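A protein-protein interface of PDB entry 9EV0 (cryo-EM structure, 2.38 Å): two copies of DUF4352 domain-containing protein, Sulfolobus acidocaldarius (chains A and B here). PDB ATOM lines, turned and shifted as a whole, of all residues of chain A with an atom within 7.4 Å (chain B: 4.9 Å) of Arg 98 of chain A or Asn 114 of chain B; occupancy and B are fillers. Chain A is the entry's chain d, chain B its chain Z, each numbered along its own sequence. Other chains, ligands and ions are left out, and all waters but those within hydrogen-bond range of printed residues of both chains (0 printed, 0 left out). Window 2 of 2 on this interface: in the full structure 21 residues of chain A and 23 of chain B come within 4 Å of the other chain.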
ATOM      1  N   ILE A  38     -30.533  26.158 -22.275  1.00  0.00           N
ATOM      2  CA  ILE A  38     -30.113  27.534 -22.445  1.00  0.00           C
ATOM      3  C   ILE A  38     -30.819  28.412 -21.406  1.00  0.00           C
ATOM      4  O   ILE A  38     -32.042  28.481 -21.372  1.00  0.00           O
ATOM      5  CB  ILE A  38     -30.371  28.026 -23.877  1.00  0.00           C
ATOM      6  CG1 ILE A  38     -29.644  27.201 -24.944  1.00  0.00           C
ATOM      7  CG2 ILE A  38     -29.954  29.479 -23.940  1.00  0.00           C
ATOM      8  CD1 ILE A  38     -28.128  27.186 -24.816  1.00  0.00           C
ATOM      9  N   GLN A  39     -30.023  29.108 -20.592  1.00  0.00           N
ATOM     10  CA  GLN A  39     -30.469  30.113 -19.638  1.00  0.00           C
ATOM     11  C   GLN A  39     -30.159  31.505 -20.190  1.00  0.00           C
ATOM     12  O   GLN A  39     -29.063  31.742 -20.695  1.00  0.00           O
ATOM     13  CB  GLN A  39     -29.750  29.901 -18.304  1.00  0.00           C
ATOM     14  CG  GLN A  39     -30.230  28.652 -17.572  1.00  0.00           C
ATOM     15  CD  GLN A  39     -29.537  28.415 -16.249  1.00  0.00           C
ATOM     16  OE1 GLN A  39     -28.717  29.215 -15.796  1.00  0.00           O
ATOM     17  NE2 GLN A  39     -29.850  27.295 -15.614  1.00  0.00           N
ATOM     18  N   VAL A  65     -26.254  34.774 -22.654  1.00  0.00           N
ATOM     19  CA  VAL A  65     -26.840  33.450 -22.711  1.00  0.00           C
ATOM     20  C   VAL A  65     -25.855  32.441 -22.111  1.00  0.00           C
ATOM     21  O   VAL A  65     -24.655  32.531 -22.341  1.00  0.00           O
ATOM     22  CB  VAL A  65     -27.226  33.146 -24.171  1.00  0.00           C
ATOM     23  CG1 VAL A  65     -26.032  32.959 -25.099  1.00  0.00           C
ATOM     24  CG2 VAL A  65     -28.125  31.948 -24.266  1.00  0.00           C
ATOM     25  N   LYS A  66     -26.365  31.489 -21.327  1.00  0.00           N
ATOM     26  CA  LYS A  66     -25.562  30.484 -20.645  1.00  0.00           C
ATOM     27  C   LYS A  66     -26.089  29.095 -21.004  1.00  0.00           C
ATOM     28  O   LYS A  66     -27.218  28.753 -20.671  1.00  0.00           O
ATOM     29  CB  LYS A  66     -25.615  30.756 -19.141  1.00  0.00           C
ATOM     30  CG  LYS A  66     -24.979  29.712 -18.239  1.00  0.00           C
ATOM     31  CD  LYS A  66     -25.033  30.129 -16.788  1.00  0.00           C
ATOM     32  CE  LYS A  66     -24.377  29.134 -15.853  1.00  0.00           C
ATOM     33  NZ  LYS A  66     -24.370  29.610 -14.447  1.00  0.00           N
ATOM     34  N   ASN A  67     -25.270  28.293 -21.682  1.00  0.00           N
ATOM     35  CA  ASN A  67     -25.633  26.925 -21.995  1.00  0.00           C
ATOM     36  C   ASN A  67     -25.201  26.026 -20.834  1.00  0.00           C
ATOM     37  O   ASN A  67     -24.010  25.817 -20.628  1.00  0.00           O
ATOM     38  CB  ASN A  67     -24.981  26.535 -23.319  1.00  0.00           C
ATOM     39  CG  ASN A  67     -25.360  25.155 -23.799  1.00  0.00           C
ATOM     40  OD1 ASN A  67     -26.041  24.403 -23.111  1.00  0.00           O
ATOM     41  ND2 ASN A  67     -24.948  24.795 -24.994  1.00  0.00           N
ATOM     42  N   THR A  68     -26.166  25.471 -20.091  1.00  0.00           N
ATOM     43  CA  THR A  68     -25.871  24.557 -18.989  1.00  0.00           C
ATOM     44  C   THR A  68     -25.909  23.084 -19.403  1.00  0.00           C
ATOM     45  O   THR A  68     -25.606  22.214 -18.592  1.00  0.00           O
ATOM     46  CB  THR A  68     -26.782  24.799 -17.782  1.00  0.00           C
ATOM     47  OG1 THR A  68     -28.150  24.638 -18.152  1.00  0.00           O
ATOM     48  CG2 THR A  68     -26.600  26.177 -17.191  1.00  0.00           C
ATOM     49  N   GLY A  69     -26.267  22.788 -20.659  1.00  0.00           N
ATOM     50  CA  GLY A  69     -26.209  21.435 -21.203  1.00  0.00           C
ATOM     51  C   GLY A  69     -24.802  21.027 -21.649  1.00  0.00           C
ATOM     52  O   GLY A  69     -23.844  21.792 -21.534  1.00  0.00           O
ATOM     53  N   THR A  70     -24.700  19.815 -22.219  1.00  0.00           N
ATOM     54  CA  THR A  70     -23.431  19.198 -22.612  1.00  0.00           C
ATOM     55  C   THR A  70     -23.194  19.223 -24.128  1.00  0.00           C
ATOM     56  O   THR A  70     -22.187  18.689 -24.599  1.00  0.00           O
ATOM     57  CB  THR A  70     -23.322  17.757 -22.095  1.00  0.00           C
ATOM     58  OG1 THR A  70     -24.485  17.040 -22.514  1.00  0.00           O
ATOM     59  CG2 THR A  70     -23.188  17.688 -20.589  1.00  0.00           C
ATOM     60  N   THR A  71     -24.108  19.842 -24.894  1.00  0.00           N
ATOM     61  CA  THR A  71     -24.034  19.938 -26.356  1.00  0.00           C
ATOM     62  C   THR A  71     -24.204  21.385 -26.819  1.00  0.00           C
ATOM     63  O   THR A  71     -24.891  22.168 -26.176  1.00  0.00           O
ATOM     64  CB  THR A  71     -25.084  19.049 -27.040  1.00  0.00           C
ATOM     65  OG1 THR A  71     -26.389  19.308 -26.516  1.00  0.00           O
ATOM     66  CG2 THR A  71     -24.758  17.579 -26.907  1.00  0.00           C
ATOM     67  N   ILE A  94     -24.313  28.258 -29.391  1.00  0.00           N
ATOM     68  CA  ILE A  94     -23.770  28.499 -28.059  1.00  0.00           C
ATOM     69  C   ILE A  94     -23.091  27.215 -27.579  1.00  0.00           C
ATOM     70  O   ILE A  94     -23.767  26.210 -27.377  1.00  0.00           O
ATOM     71  CB  ILE A  94     -24.869  28.938 -27.055  1.00  0.00           C
ATOM     72  CG1 ILE A  94     -25.731  30.123 -27.507  1.00  0.00           C
ATOM     73  CG2 ILE A  94     -24.228  29.266 -25.718  1.00  0.00           C
ATOM     74  CD1 ILE A  94     -26.966  29.777 -28.316  1.00  0.00           C
ATOM     75  N   PRO A  95     -21.752  27.202 -27.367  1.00  0.00           N
ATOM     76  CA  PRO A  95     -21.027  26.004 -26.937  1.00  0.00           C
ATOM     77  C   PRO A  95     -21.491  25.469 -25.585  1.00  0.00           C
ATOM     78  O   PRO A  95     -22.009  26.201 -24.751  1.00  0.00           O
ATOM     79  CB  PRO A  95     -19.563  26.467 -26.837  1.00  0.00           C
ATOM     80  CG  PRO A  95     -19.481  27.657 -27.770  1.00  0.00           C
ATOM     81  CD  PRO A  95     -20.836  28.317 -27.627  1.00  0.00           C
ATOM     82  N   ALA A  96     -21.282  24.169 -25.361  1.00  0.00           N
ATOM     83  CA  ALA A  96     -21.620  23.508 -24.103  1.00  0.00           C
ATOM     84  C   ALA A  96     -20.952  24.190 -22.897  1.00  0.00           C
ATOM     85  O   ALA A  96     -19.814  24.654 -22.979  1.00  0.00           O
ATOM     86  CB  ALA A  96     -21.196  22.064 -24.207  1.00  0.00           C
ATOM     87  N   GLY A  97     -21.673  24.255 -21.768  1.00  0.00           N
ATOM     88  CA  GLY A  97     -21.163  24.738 -20.487  1.00  0.00           C
ATOM     89  C   GLY A  97     -20.684  26.197 -20.443  1.00  0.00           C
ATOM     90  O   GLY A  97     -20.020  26.576 -19.480  1.00  0.00           O
ATOM     91  N   ARG A  98     -21.010  27.021 -21.453  1.00  0.00           N
ATOM     92  CA  ARG A  98     -20.390  28.332 -21.640  1.00  0.00           C
ATOM     93  C   ARG A  98     -21.395  29.483 -21.501  1.00  0.00           C
ATOM     94  O   ARG A  98     -22.553  29.351 -21.888  1.00  0.00           O
ATOM     95  CB  ARG A  98     -19.704  28.359 -23.011  1.00  0.00           C
ATOM     96  CG  ARG A  98     -18.716  29.502 -23.189  1.00  0.00           C
ATOM     97  CD  ARG A  98     -17.759  29.330 -24.356  1.00  0.00           C
ATOM     98  NE  ARG A  98     -16.903  28.149 -24.247  1.00  0.00           N
ATOM     99  CZ  ARG A  98     -15.823  28.033 -23.473  1.00  0.00           C
ATOM    100  NH1 ARG A  98     -15.136  26.902 -23.471  1.00  0.00           N
ATOM    101  NH2 ARG A  98     -15.431  29.034 -22.702  1.00  0.00           N
ATOM    102  N   THR A  99     -20.928  30.620 -20.959  1.00  0.00           N
ATOM    103  CA  THR A  99     -21.686  31.869 -20.914  1.00  0.00           C
ATOM    104  C   THR A  99     -21.104  32.849 -21.932  1.00  0.00           C
ATOM    105  O   THR A  99     -19.895  33.074 -21.949  1.00  0.00           O
ATOM    106  CB  THR A  99     -21.658  32.528 -19.526  1.00  0.00           C
ATOM    107  OG1 THR A  99     -22.082  31.590 -18.541  1.00  0.00           O
ATOM    108  CG2 THR A  99     -22.557  33.742 -19.425  1.00  0.00           C
ATOM    109  N   GLN A 100     -21.962  33.435 -22.782  1.00  0.00           N
ATOM    110  CA  GLN A 100     -21.549  34.355 -23.837  1.00  0.00           C
ATOM    111  C   GLN A 100     -22.578  35.464 -24.020  1.00  0.00           C
ATOM    112  O   GLN A 100     -23.771  35.230 -23.872  1.00  0.00           O
ATOM    113  CB  GLN A 100     -21.450  33.633 -25.184  1.00  0.00           C
ATOM    114  CG  GLN A 100     -20.372  32.557 -25.258  1.00  0.00           C
ATOM    115  CD  GLN A 100     -20.272  31.958 -26.640  1.00  0.00           C
ATOM    116  OE1 GLN A 100     -21.273  31.728 -27.318  1.00  0.00           O
ATOM    117  NE2 GLN A 100     -19.046  31.687 -27.064  1.00  0.00           N
ATOM    118  N   LYS B 112     -16.247  16.467 -27.069  1.00  0.00           N
ATOM    119  CA  LYS B 112     -15.619  17.125 -25.932  1.00  0.00           C
ATOM    120  C   LYS B 112     -16.666  17.899 -25.127  1.00  0.00           C
ATOM    121  O   LYS B 112     -17.026  19.014 -25.491  1.00  0.00           O
ATOM    122  CB  LYS B 112     -14.460  18.012 -26.407  1.00  0.00           C
ATOM    123  CG  LYS B 112     -13.767  18.830 -25.322  1.00  0.00           C
ATOM    124  CD  LYS B 112     -13.263  18.004 -24.149  1.00  0.00           C
ATOM    125  CE  LYS B 112     -12.490  18.796 -23.110  1.00  0.00           C
ATOM    126  NZ  LYS B 112     -13.335  19.790 -22.407  1.00  0.00           N
ATOM    127  N   PRO B 113     -17.200  17.333 -24.018  1.00  0.00           N
ATOM    128  CA  PRO B 113     -18.134  18.048 -23.155  1.00  0.00           C
ATOM    129  C   PRO B 113     -17.390  19.073 -22.300  1.00  0.00           C
ATOM    130  O   PRO B 113     -16.160  19.068 -22.199  1.00  0.00           O
ATOM    131  CB  PRO B 113     -18.749  16.943 -22.279  1.00  0.00           C
ATOM    132  CG  PRO B 113     -17.645  15.917 -22.177  1.00  0.00           C
ATOM    133  CD  PRO B 113     -16.914  15.989 -23.506  1.00  0.00           C
ATOM    134  N   ASN B 114     -18.177  19.959 -21.693  1.00  0.00           N
ATOM    135  CA  ASN B 114     -17.666  21.037 -20.872  1.00  0.00           C
ATOM    136  C   ASN B 114     -18.686  21.304 -19.767  1.00  0.00           C
ATOM    137  O   ASN B 114     -19.689  21.966 -20.008  1.00  0.00           O
ATOM    138  CB  ASN B 114     -17.365  22.248 -21.754  1.00  0.00           C
ATOM    139  CG  ASN B 114     -16.853  23.438 -20.979  1.00  0.00           C
ATOM    140  OD1 ASN B 114     -15.924  23.317 -20.185  1.00  0.00           O
ATOM    141  ND2 ASN B 114     -17.430  24.603 -21.224  1.00  0.00           N
ATOM    142  N   PHE B 115     -18.463  20.734 -18.578  1.00  0.00           N
ATOM    143  CA  PHE B 115     -19.362  20.946 -17.457  1.00  0.00           C
ATOM    144  C   PHE B 115     -19.085  22.297 -16.788  1.00  0.00           C
ATOM    145  O   PHE B 115     -17.945  22.745 -16.741  1.00  0.00           O
ATOM    146  CB  PHE B 115     -19.209  19.791 -16.474  1.00  0.00           C
ATOM    147  CG  PHE B 115     -19.385  18.407 -17.050  1.00  0.00           C
ATOM    148  CD1 PHE B 115     -20.651  17.919 -17.353  1.00  0.00           C
ATOM    149  CD2 PHE B 115     -18.288  17.570 -17.239  1.00  0.00           C
ATOM    150  CE1 PHE B 115     -20.820  16.630 -17.849  1.00  0.00           C
ATOM    151  CE2 PHE B 115     -18.453  16.275 -17.730  1.00  0.00           C
ATOM    152  CZ  PHE B 115     -19.721  15.807 -18.035  1.00  0.00           C
ATOM    153  N   SER B 116     -20.135  22.935 -16.250  1.00  0.00           N
ATOM    154  CA  SER B 116     -20.051  24.222 -15.561  1.00  0.00           C
ATOM    155  C   SER B 116     -20.256  24.048 -14.052  1.00  0.00           C
ATOM    156  O   SER B 116     -21.143  23.310 -13.639  1.00  0.00           O
ATOM    157  CB  SER B 116     -21.034  25.207 -16.158  1.00  0.00           C
ATOM    158  OG  SER B 116     -22.358  24.696 -16.150  1.00  0.00           O
ATOM    159  N   TYR B 121     -26.352  17.673 -13.998  1.00  0.00           N
ATOM    160  CA  TYR B 121     -26.357  16.835 -15.189  1.00  0.00           C
ATOM    161  C   TYR B 121     -27.000  15.505 -14.812  1.00  0.00           C
ATOM    162  O   TYR B 121     -26.712  14.975 -13.742  1.00  0.00           O
ATOM    163  CB  TYR B 121     -24.913  16.638 -15.675  1.00  0.00           C
ATOM    164  CG  TYR B 121     -24.266  17.958 -16.015  1.00  0.00           C
ATOM    165  CD1 TYR B 121     -24.425  18.522 -17.276  1.00  0.00           C
ATOM    166  CD2 TYR B 121     -23.579  18.690 -15.052  1.00  0.00           C
ATOM    167  CE1 TYR B 121     -23.919  19.782 -17.566  1.00  0.00           C
ATOM    168  CE2 TYR B 121     -23.071  19.954 -15.326  1.00  0.00           C
ATOM    169  CZ  TYR B 121     -23.251  20.504 -16.590  1.00  0.00           C
ATOM    170  OH  TYR B 121     -22.789  21.757 -16.892  1.00  0.00           O
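The backbone NH (N) of Ser 116 of chain B is in hydrogen-bond range of the side-chain hydroxyl (OH) of Tyr 121 of chain B (3.0 Å). The backbone carbonyl oxygen (O) of Asn 67 of chain A lies within hydrogen-bond range of the backbone NH (N) of Gly 97 of chain A. The backbone carbonyl oxygen of Arg 98 of chain A lies within hydrogen-bond range of the backbone NH of Asn 67 of chain A (2.9 Å). The backbone carbonyl oxygen of Gly 69 of chain A is in hydrogen-bond range of the backbone NH of Gly 97 of chain A, 3.3 Å away.
No position is printed for both chains.
The backbone carbonyl oxygen (O) of Ala 96 of chain A sits at hydrogen-bond distance from the side-chain amide nitrogen (ND2) of Asn 114 of chain B, 3.0 Å away. The side-chain hydroxyl (OH) of Tyr 121 of chain B sits close to the backbone carbonyl oxygen (O) of Thr 68 of chain A.
Of the 16 printed residues of chain A, 5 touch a printed residue of chain B. Along chain A the printed residues that touch a printed residue of chain B span positions 68 to 98. Of the 6 printed residues of chain B, 4 touch a printed residue of chain A. Printed residues of chain B that touch a printed residue of chain A: Asn 114, Phe 115, Ser 116 and Tyr 121.
Printed residues of chain B within 4 Å of Thr 68 of chain A: Tyr 121 (3.1 Å). Of the printed residues of chain B, Gly 97 of chain A touches Asn 114 and Ser 116. Of chain B, only Asn 114 (3.9 Å) comes within 4 Å of Arg 98 of chain A. Asn 114 of chain B touches three residues of chain A. Printed residues of chain A within 4 Å of Ser 116 of chain B: Gly 97 (3.7 Å). The nearest printed residue of chain B that does not touch Arg 98 of chain A is Ser 116 of chain B (5.6 Å). The nearest residue of chain A that does not touch Asn 114 of chain B is Gly 69 of chain A (4.4 Å).
Among the printed residues, merely in contact across the chains: Thr 70 of chain A with Phe 115 of chain B (3.8 Å), Thr 70 of chain A with Tyr 121 of chain B (3.6 Å), Gly 97 of chain A with Asn 114 of chain B (3.2 Å), Gly 97 of chain A with Ser 116 of chain B (3.7 Å) and Arg 98 of chain A with Asn 114 of chain B (3.9 Å).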
